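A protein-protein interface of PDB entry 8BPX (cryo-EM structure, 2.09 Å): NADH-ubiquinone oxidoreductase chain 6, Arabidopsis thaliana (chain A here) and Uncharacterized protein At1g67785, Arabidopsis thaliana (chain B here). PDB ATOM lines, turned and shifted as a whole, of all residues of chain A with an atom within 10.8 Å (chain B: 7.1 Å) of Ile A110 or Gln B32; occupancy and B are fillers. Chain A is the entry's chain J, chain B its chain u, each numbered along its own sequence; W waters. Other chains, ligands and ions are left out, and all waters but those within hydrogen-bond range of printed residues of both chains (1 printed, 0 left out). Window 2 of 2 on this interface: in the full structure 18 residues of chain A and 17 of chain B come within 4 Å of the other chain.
OE1 of Gln B32 sits close to O of Ile B28 (3.3 Å).
Printed residues of chain B within 4 Å of Phe A103: Ile B28. Of the printed residues of chain B, Asn A107 touches Lys B35. Of the printed residues of chain B, Ile A110 touches Gln B32. Printed residues of chain B within 4 Å of Pro A111: Ala B29 (3.6 Å). Printed residues of chain B within 4 Å of Leu A113: Ala B29 (3.7 Å) and Leu B30 (3.7 Å). Of chain A, only Pro A111 (3.6 Å) and Leu A113 (3.7 Å) come within 4 Å of Ala B29. Of the printed residues of chain A, Leu B30 touches Leu A113. Of the printed residues of chain A, Gln B32 touches Ile A110. No residue of chain A comes within 4 Å of Asp B33. No residue of chain A comes within 4 Å of Glu B34. Of the printed residues of chain A, Lys B35 touches Asn A107. No residue of chain A comes within 4 Å of Gln B36.
Among the printed residues, merely in contact across the chains: Phe A103 with Ile B28, Asp A106 with Ile B28, Ile A110 with Gln B32, Pro A111 with Ala B29, Leu A113 with Ala B29 and Leu A113 with Leu B30.
Water W1 bridges the side-chain carboxylate (OD2) of Asp A106 (3.2 Å) and the backbone NH (N) of Ala B29 (3.3 Å).
Hydrophobic or aromatic side chains of chain A that line the printed part of chain B: Phe A103, Ile A110, Pro A111 and Leu A113. Among the printed residues, no Asp or Glu carboxylate lies within 4 Å of a Lys or Arg side-chain nitrogen of the other chain.
OD1 of Asn A107 lies within hydrogen-bond range of NZ of Lys B35, 3.1 Å away.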
ATOM      1  N   TRP A  99      -6.210 -27.937  -0.393  1.00  0.00           N
ATOM      2  CA  TRP A  99      -5.356 -26.844  -0.851  1.00  0.00           C
ATOM      3  C   TRP A  99      -4.601 -27.204  -2.121  1.00  0.00           C
ATOM      4  O   TRP A  99      -4.338 -26.338  -2.962  1.00  0.00           O
ATOM      5  CB  TRP A  99      -4.371 -26.456   0.250  1.00  0.00           C
ATOM      6  CG  TRP A  99      -3.297 -25.522  -0.219  1.00  0.00           C
ATOM      7  CD1 TRP A  99      -1.958 -25.764  -0.226  1.00  0.00           C
ATOM      8  CD2 TRP A  99      -3.470 -24.207  -0.771  1.00  0.00           C
ATOM      9  NE1 TRP A  99      -1.281 -24.684  -0.735  1.00  0.00           N
ATOM     10  CE2 TRP A  99      -2.186 -23.715  -1.078  1.00  0.00           C
ATOM     11  CE3 TRP A  99      -4.581 -23.398  -1.029  1.00  0.00           C
ATOM     12  CZ2 TRP A  99      -1.982 -22.452  -1.630  1.00  0.00           C
ATOM     13  CZ3 TRP A  99      -4.376 -22.145  -1.577  1.00  0.00           C
ATOM     14  CH2 TRP A  99      -3.088 -21.684  -1.871  1.00  0.00           C
ATOM     15  N   PHE A 103      -7.307 -26.869  -6.551  1.00  0.00           N
ATOM     16  CA  PHE A 103      -6.726 -25.719  -7.238  1.00  0.00           C
ATOM     17  C   PHE A 103      -5.614 -26.114  -8.197  1.00  0.00           C
ATOM     18  O   PHE A 103      -4.861 -25.244  -8.646  1.00  0.00           O
ATOM     19  CB  PHE A 103      -6.200 -24.707  -6.214  1.00  0.00           C
ATOM     20  CG  PHE A 103      -7.200 -24.349  -5.151  1.00  0.00           C
ATOM     21  CD1 PHE A 103      -8.290 -23.548  -5.450  1.00  0.00           C
ATOM     22  CD2 PHE A 103      -7.063 -24.832  -3.860  1.00  0.00           C
ATOM     23  CE1 PHE A 103      -9.219 -23.224  -4.477  1.00  0.00           C
ATOM     24  CE2 PHE A 103      -7.989 -24.513  -2.885  1.00  0.00           C
ATOM     25  CZ  PHE A 103      -9.070 -23.709  -3.195  1.00  0.00           C
ATOM     26  N   ILE A 104      -5.494 -27.403  -8.522  1.00  0.00           N
ATOM     27  CA  ILE A 104      -4.406 -27.880  -9.370  1.00  0.00           C
ATOM     28  C   ILE A 104      -4.528 -27.327 -10.784  1.00  0.00           C
ATOM     29  O   ILE A 104      -3.517 -27.060 -11.442  1.00  0.00           O
ATOM     30  CB  ILE A 104      -4.376 -29.421  -9.344  1.00  0.00           C
ATOM     31  CG1 ILE A 104      -3.348 -29.988 -10.318  1.00  0.00           C
ATOM     32  CG2 ILE A 104      -5.730 -29.979  -9.644  1.00  0.00           C
ATOM     33  CD1 ILE A 104      -2.759 -31.297  -9.866  1.00  0.00           C
ATOM     34  N   LEU A 105      -5.755 -27.138 -11.270  1.00  0.00           N
ATOM     35  CA  LEU A 105      -5.975 -26.620 -12.614  1.00  0.00           C
ATOM     36  C   LEU A 105      -5.801 -25.109 -12.714  1.00  0.00           C
ATOM     37  O   LEU A 105      -5.736 -24.587 -13.832  1.00  0.00           O
ATOM     38  CB  LEU A 105      -7.380 -26.991 -13.104  1.00  0.00           C
ATOM     39  CG  LEU A 105      -7.802 -28.460 -13.164  1.00  0.00           C
ATOM     40  CD1 LEU A 105      -9.015 -28.629 -14.069  1.00  0.00           C
ATOM     41  CD2 LEU A 105      -6.667 -29.343 -13.638  1.00  0.00           C
ATOM     42  N   ASP A 106      -5.723 -24.398 -11.586  1.00  0.00           N
ATOM     43  CA  ASP A 106      -5.784 -22.939 -11.620  1.00  0.00           C
ATOM     44  C   ASP A 106      -4.605 -22.331 -12.372  1.00  0.00           C
ATOM     45  O   ASP A 106      -4.776 -21.364 -13.120  1.00  0.00           O
ATOM     46  CB  ASP A 106      -5.866 -22.387 -10.198  1.00  0.00           C
ATOM     47  CG  ASP A 106      -7.186 -22.719  -9.526  1.00  0.00           C
ATOM     48  OD1 ASP A 106      -7.726 -23.813  -9.788  1.00  0.00           O
ATOM     49  OD2 ASP A 106      -7.686 -21.887  -8.743  1.00  0.00           O
ATOM     50  N   ASN A 107      -3.402 -22.875 -12.187  1.00  0.00           N
ATOM     51  CA  ASN A 107      -2.237 -22.308 -12.861  1.00  0.00           C
ATOM     52  C   ASN A 107      -2.201 -22.688 -14.336  1.00  0.00           C
ATOM     53  O   ASN A 107      -1.758 -21.894 -15.173  1.00  0.00           O
ATOM     54  CB  ASN A 107      -0.956 -22.758 -12.164  1.00  0.00           C
ATOM     55  CG  ASN A 107      -0.616 -21.897 -10.971  1.00  0.00           C
ATOM     56  OD1 ASN A 107      -1.495 -21.291 -10.358  1.00  0.00           O
ATOM     57  ND2 ASN A 107       0.665 -21.839 -10.629  1.00  0.00           N
ATOM     58  N   GLU A 108      -2.659 -23.892 -14.669  1.00  0.00           N
ATOM     59  CA  GLU A 108      -2.675 -24.319 -16.062  1.00  0.00           C
ATOM     60  C   GLU A 108      -3.908 -23.800 -16.788  1.00  0.00           C
ATOM     61  O   GLU A 108      -3.807 -23.326 -17.925  1.00  0.00           O
ATOM     62  CB  GLU A 108      -2.613 -25.842 -16.144  1.00  0.00           C
ATOM     63  CG  GLU A 108      -2.223 -26.371 -17.510  1.00  0.00           C
ATOM     64  CD  GLU A 108      -0.750 -26.171 -17.804  1.00  0.00           C
ATOM     65  OE1 GLU A 108      -0.377 -25.070 -18.260  1.00  0.00           O
ATOM     66  OE2 GLU A 108       0.036 -27.113 -17.576  1.00  0.00           O
ATOM     67  N   SER A 109      -5.071 -23.881 -16.151  1.00  0.00           N
ATOM     68  CA  SER A 109      -6.339 -23.468 -16.746  1.00  0.00           C
ATOM     69  C   SER A 109      -6.858 -22.277 -15.947  1.00  0.00           C
ATOM     70  O   SER A 109      -7.643 -22.431 -15.009  1.00  0.00           O
ATOM     71  CB  SER A 109      -7.326 -24.620 -16.757  1.00  0.00           C
ATOM     72  OG  SER A 109      -6.904 -25.628 -17.658  1.00  0.00           O
ATOM     73  N   ILE A 110      -6.411 -21.089 -16.325  1.00  0.00           N
ATOM     74  CA  ILE A 110      -6.811 -19.862 -15.633  1.00  0.00           C
ATOM     75  C   ILE A 110      -8.225 -19.492 -16.070  1.00  0.00           C
ATOM     76  O   ILE A 110      -8.487 -19.401 -17.277  1.00  0.00           O
ATOM     77  CB  ILE A 110      -5.828 -18.737 -15.933  1.00  0.00           C
ATOM     78  CG1 ILE A 110      -4.497 -19.003 -15.232  1.00  0.00           C
ATOM     79  CG2 ILE A 110      -6.399 -17.396 -15.497  1.00  0.00           C
ATOM     80  CD1 ILE A 110      -3.329 -18.343 -15.882  1.00  0.00           C
ATOM     81  N   PRO A 111      -9.148 -19.278 -15.140  1.00  0.00           N
ATOM     82  CA  PRO A 111     -10.525 -18.961 -15.529  1.00  0.00           C
ATOM     83  C   PRO A 111     -10.637 -17.602 -16.200  1.00  0.00           C
ATOM     84  O   PRO A 111      -9.875 -16.673 -15.924  1.00  0.00           O
ATOM     85  CB  PRO A 111     -11.284 -18.985 -14.199  1.00  0.00           C
ATOM     86  CG  PRO A 111     -10.257 -18.706 -13.175  1.00  0.00           C
ATOM     87  CD  PRO A 111      -8.978 -19.313 -13.679  1.00  0.00           C
ATOM     88  N   LEU A 112     -11.610 -17.501 -17.098  1.00  0.00           N
ATOM     89  CA  LEU A 112     -11.965 -16.229 -17.708  1.00  0.00           C
ATOM     90  C   LEU A 112     -12.949 -15.503 -16.798  1.00  0.00           C
ATOM     91  O   LEU A 112     -14.071 -15.975 -16.590  1.00  0.00           O
ATOM     92  CB  LEU A 112     -12.567 -16.457 -19.091  1.00  0.00           C
ATOM     93  CG  LEU A 112     -12.853 -15.230 -19.953  1.00  0.00           C
ATOM     94  CD1 LEU A 112     -11.559 -14.559 -20.395  1.00  0.00           C
ATOM     95  CD2 LEU A 112     -13.706 -15.614 -21.149  1.00  0.00           C
ATOM     96  N   LEU A 113     -12.532 -14.368 -16.251  1.00  0.00           N
ATOM     97  CA  LEU A 113     -13.416 -13.599 -15.384  1.00  0.00           C
ATOM     98  C   LEU A 113     -14.555 -13.004 -16.206  1.00  0.00           C
ATOM     99  O   LEU A 113     -14.302 -12.345 -17.220  1.00  0.00           O
ATOM    100  CB  LEU A 113     -12.643 -12.498 -14.660  1.00  0.00           C
ATOM    101  CG  LEU A 113     -11.401 -12.977 -13.908  1.00  0.00           C
ATOM    102  CD1 LEU A 113     -10.678 -11.826 -13.239  1.00  0.00           C
ATOM    103  CD2 LEU A 113     -11.783 -14.039 -12.887  1.00  0.00           C
ATOM    104  N   PRO A 114     -15.809 -13.211 -15.809  1.00  0.00           N
ATOM    105  CA  PRO A 114     -16.938 -12.687 -16.596  1.00  0.00           C
ATOM    106  C   PRO A 114     -17.061 -11.182 -16.410  1.00  0.00           C
ATOM    107  O   PRO A 114     -17.201 -10.692 -15.287  1.00  0.00           O
ATOM    108  CB  PRO A 114     -18.145 -13.435 -16.023  1.00  0.00           C
ATOM    109  CG  PRO A 114     -17.755 -13.753 -14.619  1.00  0.00           C
ATOM    110  CD  PRO A 114     -16.253 -13.869 -14.568  1.00  0.00           C
ATOM    111  N   TRP B  27     -10.486 -14.831  -6.776  1.00  0.00           N
ATOM    112  CA  TRP B  27      -9.288 -14.282  -6.143  1.00  0.00           C
ATOM    113  C   TRP B  27      -8.016 -14.835  -6.773  1.00  0.00           C
ATOM    114  O   TRP B  27      -7.084 -14.081  -7.077  1.00  0.00           O
ATOM    115  CB  TRP B  27      -9.294 -14.568  -4.644  1.00  0.00           C
ATOM    116  CG  TRP B  27      -8.351 -13.692  -3.894  1.00  0.00           C
ATOM    117  CD1 TRP B  27      -8.588 -12.435  -3.432  1.00  0.00           C
ATOM    118  CD2 TRP B  27      -6.999 -14.002  -3.541  1.00  0.00           C
ATOM    119  NE1 TRP B  27      -7.474 -11.945  -2.800  1.00  0.00           N
ATOM    120  CE2 TRP B  27      -6.483 -12.890  -2.851  1.00  0.00           C
ATOM    121  CE3 TRP B  27      -6.178 -15.116  -3.734  1.00  0.00           C
ATOM    122  CZ2 TRP B  27      -5.183 -12.855  -2.357  1.00  0.00           C
ATOM    123  CZ3 TRP B  27      -4.885 -15.082  -3.239  1.00  0.00           C
ATOM    124  CH2 TRP B  27      -4.401 -13.958  -2.561  1.00  0.00           C
ATOM    125  N   ILE B  28      -7.956 -16.153  -6.967  1.00  0.00           N
ATOM    126  CA  ILE B  28      -6.745 -16.759  -7.519  1.00  0.00           C
ATOM    127  C   ILE B  28      -6.487 -16.243  -8.929  1.00  0.00           C
ATOM    128  O   ILE B  28      -5.345 -15.937  -9.294  1.00  0.00           O
ATOM    129  CB  ILE B  28      -6.839 -18.294  -7.481  1.00  0.00           C
ATOM    130  CG1 ILE B  28      -6.705 -18.797  -6.044  1.00  0.00           C
ATOM    131  CG2 ILE B  28      -5.758 -18.918  -8.351  1.00  0.00           C
ATOM    132  CD1 ILE B  28      -7.416 -20.093  -5.791  1.00  0.00           C
ATOM    133  N   ALA B  29      -7.540 -16.130  -9.741  1.00  0.00           N
ATOM    134  CA  ALA B  29      -7.375 -15.614 -11.096  1.00  0.00           C
ATOM    135  C   ALA B  29      -6.879 -14.171 -11.089  1.00  0.00           C
ATOM    136  O   ALA B  29      -6.027 -13.798 -11.905  1.00  0.00           O
ATOM    137  CB  ALA B  29      -8.689 -15.723 -11.868  1.00  0.00           C
ATOM    138  N   LEU B  30      -7.395 -13.345 -10.176  1.00  0.00           N
ATOM    139  CA  LEU B  30      -7.014 -11.935 -10.160  1.00  0.00           C
ATOM    140  C   LEU B  30      -5.553 -11.715  -9.789  1.00  0.00           C
ATOM    141  O   LEU B  30      -5.017 -10.639 -10.066  1.00  0.00           O
ATOM    142  CB  LEU B  30      -7.909 -11.149  -9.200  1.00  0.00           C
ATOM    143  CG  LEU B  30      -9.302 -10.804  -9.726  1.00  0.00           C
ATOM    144  CD1 LEU B  30     -10.264 -10.554  -8.582  1.00  0.00           C
ATOM    145  CD2 LEU B  30      -9.243  -9.602 -10.649  1.00  0.00           C
ATOM    146  N   HIS B  31      -4.892 -12.701  -9.185  1.00  0.00           N
ATOM    147  CA  HIS B  31      -3.515 -12.557  -8.737  1.00  0.00           C
ATOM    148  C   HIS B  31      -2.516 -13.279  -9.632  1.00  0.00           C
ATOM    149  O   HIS B  31      -1.384 -13.527  -9.206  1.00  0.00           O
ATOM    150  CB  HIS B  31      -3.379 -13.039  -7.292  1.00  0.00           C
ATOM    151  CG  HIS B  31      -3.927 -12.074  -6.288  1.00  0.00           C
ATOM    152  ND1 HIS B  31      -5.278 -11.866  -6.115  1.00  0.00           N
ATOM    153  CD2 HIS B  31      -3.304 -11.250  -5.413  1.00  0.00           C
ATOM    154  CE1 HIS B  31      -5.464 -10.957  -5.174  1.00  0.00           C
ATOM    155  NE2 HIS B  31      -4.282 -10.569  -4.730  1.00  0.00           N
ATOM    156  N   GLN B  32      -2.908 -13.626 -10.860  1.00  0.00           N
ATOM    157  CA  GLN B  32      -1.966 -14.261 -11.777  1.00  0.00           C
ATOM    158  C   GLN B  32      -0.811 -13.325 -12.120  1.00  0.00           C
ATOM    159  O   GLN B  32       0.348 -13.750 -12.169  1.00  0.00           O
ATOM    160  CB  GLN B  32      -2.685 -14.706 -13.051  1.00  0.00           C
ATOM    161  CG  GLN B  32      -3.489 -15.987 -12.915  1.00  0.00           C
ATOM    162  CD  GLN B  32      -2.712 -17.103 -12.244  1.00  0.00           C
ATOM    163  OE1 GLN B  32      -2.943 -17.420 -11.079  1.00  0.00           O
ATOM    164  NE2 GLN B  32      -1.786 -17.705 -12.978  1.00  0.00           N
ATOM    165  N   ASP B  33      -1.112 -12.048 -12.367  1.00  0.00           N
ATOM    166  CA  ASP B  33      -0.081 -11.110 -12.806  1.00  0.00           C
ATOM    167  C   ASP B  33       0.972 -10.881 -11.728  1.00  0.00           C
ATOM    168  O   ASP B  33       2.171 -10.864 -12.023  1.00  0.00           O
ATOM    169  CB  ASP B  33      -0.722  -9.789 -13.218  1.00  0.00           C
ATOM    170  CG  ASP B  33      -2.041  -9.982 -13.938  1.00  0.00           C
ATOM    171  OD1 ASP B  33      -2.024 -10.236 -15.160  1.00  0.00           O
ATOM    172  OD2 ASP B  33      -3.098  -9.877 -13.279  1.00  0.00           O
ATOM    173  N   GLU B  34       0.546 -10.693 -10.476  1.00  0.00           N
ATOM    174  CA  GLU B  34       1.506 -10.494  -9.394  1.00  0.00           C
ATOM    175  C   GLU B  34       2.375 -11.729  -9.190  1.00  0.00           C
ATOM    176  O   GLU B  34       3.581 -11.615  -8.946  1.00  0.00           O
ATOM    177  CB  GLU B  34       0.782 -10.132  -8.099  1.00  0.00           C
ATOM    178  CG  GLU B  34       0.288  -8.692  -8.021  1.00  0.00           C
ATOM    179  CD  GLU B  34      -0.778  -8.373  -9.053  1.00  0.00           C
ATOM    180  OE1 GLU B  34      -1.973  -8.576  -8.759  1.00  0.00           O
ATOM    181  OE2 GLU B  34      -0.415  -7.915 -10.158  1.00  0.00           O
ATOM    182  N   LYS B  35       1.775 -12.919  -9.273  1.00  0.00           N
ATOM    183  CA  LYS B  35       2.555 -14.145  -9.151  1.00  0.00           C
ATOM    184  C   LYS B  35       3.572 -14.258 -10.277  1.00  0.00           C
ATOM    185  O   LYS B  35       4.718 -14.665 -10.053  1.00  0.00           O
ATOM    186  CB  LYS B  35       1.627 -15.360  -9.138  1.00  0.00           C
ATOM    187  CG  LYS B  35       2.342 -16.680  -8.936  1.00  0.00           C
ATOM    188  CD  LYS B  35       1.666 -17.800  -9.712  1.00  0.00           C
ATOM    189  CE  LYS B  35       0.327 -18.164  -9.097  1.00  0.00           C
ATOM    190  NZ  LYS B  35       0.306 -19.568  -8.598  1.00  0.00           N
ATOM    191  N   GLN B  36       3.173 -13.891 -11.497  1.00  0.00           N
ATOM    192  CA  GLN B  36       4.114 -13.882 -12.612  1.00  0.00           C
ATOM    193  C   GLN B  36       5.243 -12.889 -12.371  1.00  0.00           C
ATOM    194  O   GLN B  36       6.406 -13.178 -12.668  1.00  0.00           O
ATOM    195  CB  GLN B  36       3.382 -13.552 -13.909  1.00  0.00           C
ATOM    196  CG  GLN B  36       3.227 -14.728 -14.855  1.00  0.00           C
ATOM    197  CD  GLN B  36       2.974 -14.287 -16.280  1.00  0.00           C
ATOM    198  OE1 GLN B  36       3.124 -13.112 -16.613  1.00  0.00           O
ATOM    199  NE2 GLN B  36       2.588 -15.228 -17.132  1.00  0.00           N
ATOM    200  N   GLU B  37       4.915 -11.709 -11.845  1.00  0.00           N
ATOM    201  CA  GLU B  37       5.940 -10.708 -11.562  1.00  0.00           C
ATOM    202  C   GLU B  37       6.928 -11.213 -10.518  1.00  0.00           C
ATOM    203  O   GLU B  37       8.143 -11.029 -10.658  1.00  0.00           O
ATOM    204  CB  GLU B  37       5.280  -9.411 -11.099  1.00  0.00           C
ATOM    205  CG  GLU B  37       6.234  -8.243 -10.927  1.00  0.00           C
ATOM    206  CD  GLU B  37       5.552  -7.025 -10.335  1.00  0.00           C
ATOM    207  OE1 GLU B  37       4.360  -7.126  -9.978  1.00  0.00           O
ATOM    208  OE2 GLU B  37       6.208  -5.968 -10.229  1.00  0.00           O
ATOM    209  N   ARG B  38       6.422 -11.852  -9.461  1.00  0.00           N
ATOM    210  CA  ARG B  38       7.296 -12.417  -8.438  1.00  0.00           C
ATOM    211  C   ARG B  38       8.183 -13.510  -9.020  1.00  0.00           C
ATOM    212  O   ARG B  38       9.387 -13.569  -8.732  1.00  0.00           O
ATOM    213  CB  ARG B  38       6.457 -12.962  -7.284  1.00  0.00           C
ATOM    214  CG  ARG B  38       7.184 -13.030  -5.952  1.00  0.00           C
ATOM    215  CD  ARG B  38       6.858 -14.319  -5.213  1.00  0.00           C
ATOM    216  NE  ARG B  38       5.460 -14.709  -5.366  1.00  0.00           N
ATOM    217  CZ  ARG B  38       4.450 -14.157  -4.708  1.00  0.00           C
ATOM    218  NH1 ARG B  38       4.642 -13.177  -3.838  1.00  0.00           N
ATOM    219  NH2 ARG B  38       3.215 -14.599  -4.926  1.00  0.00           N
HETATM  220  O   HOH W   1      -8.148 -19.252 -10.486  1.00  0.00           O
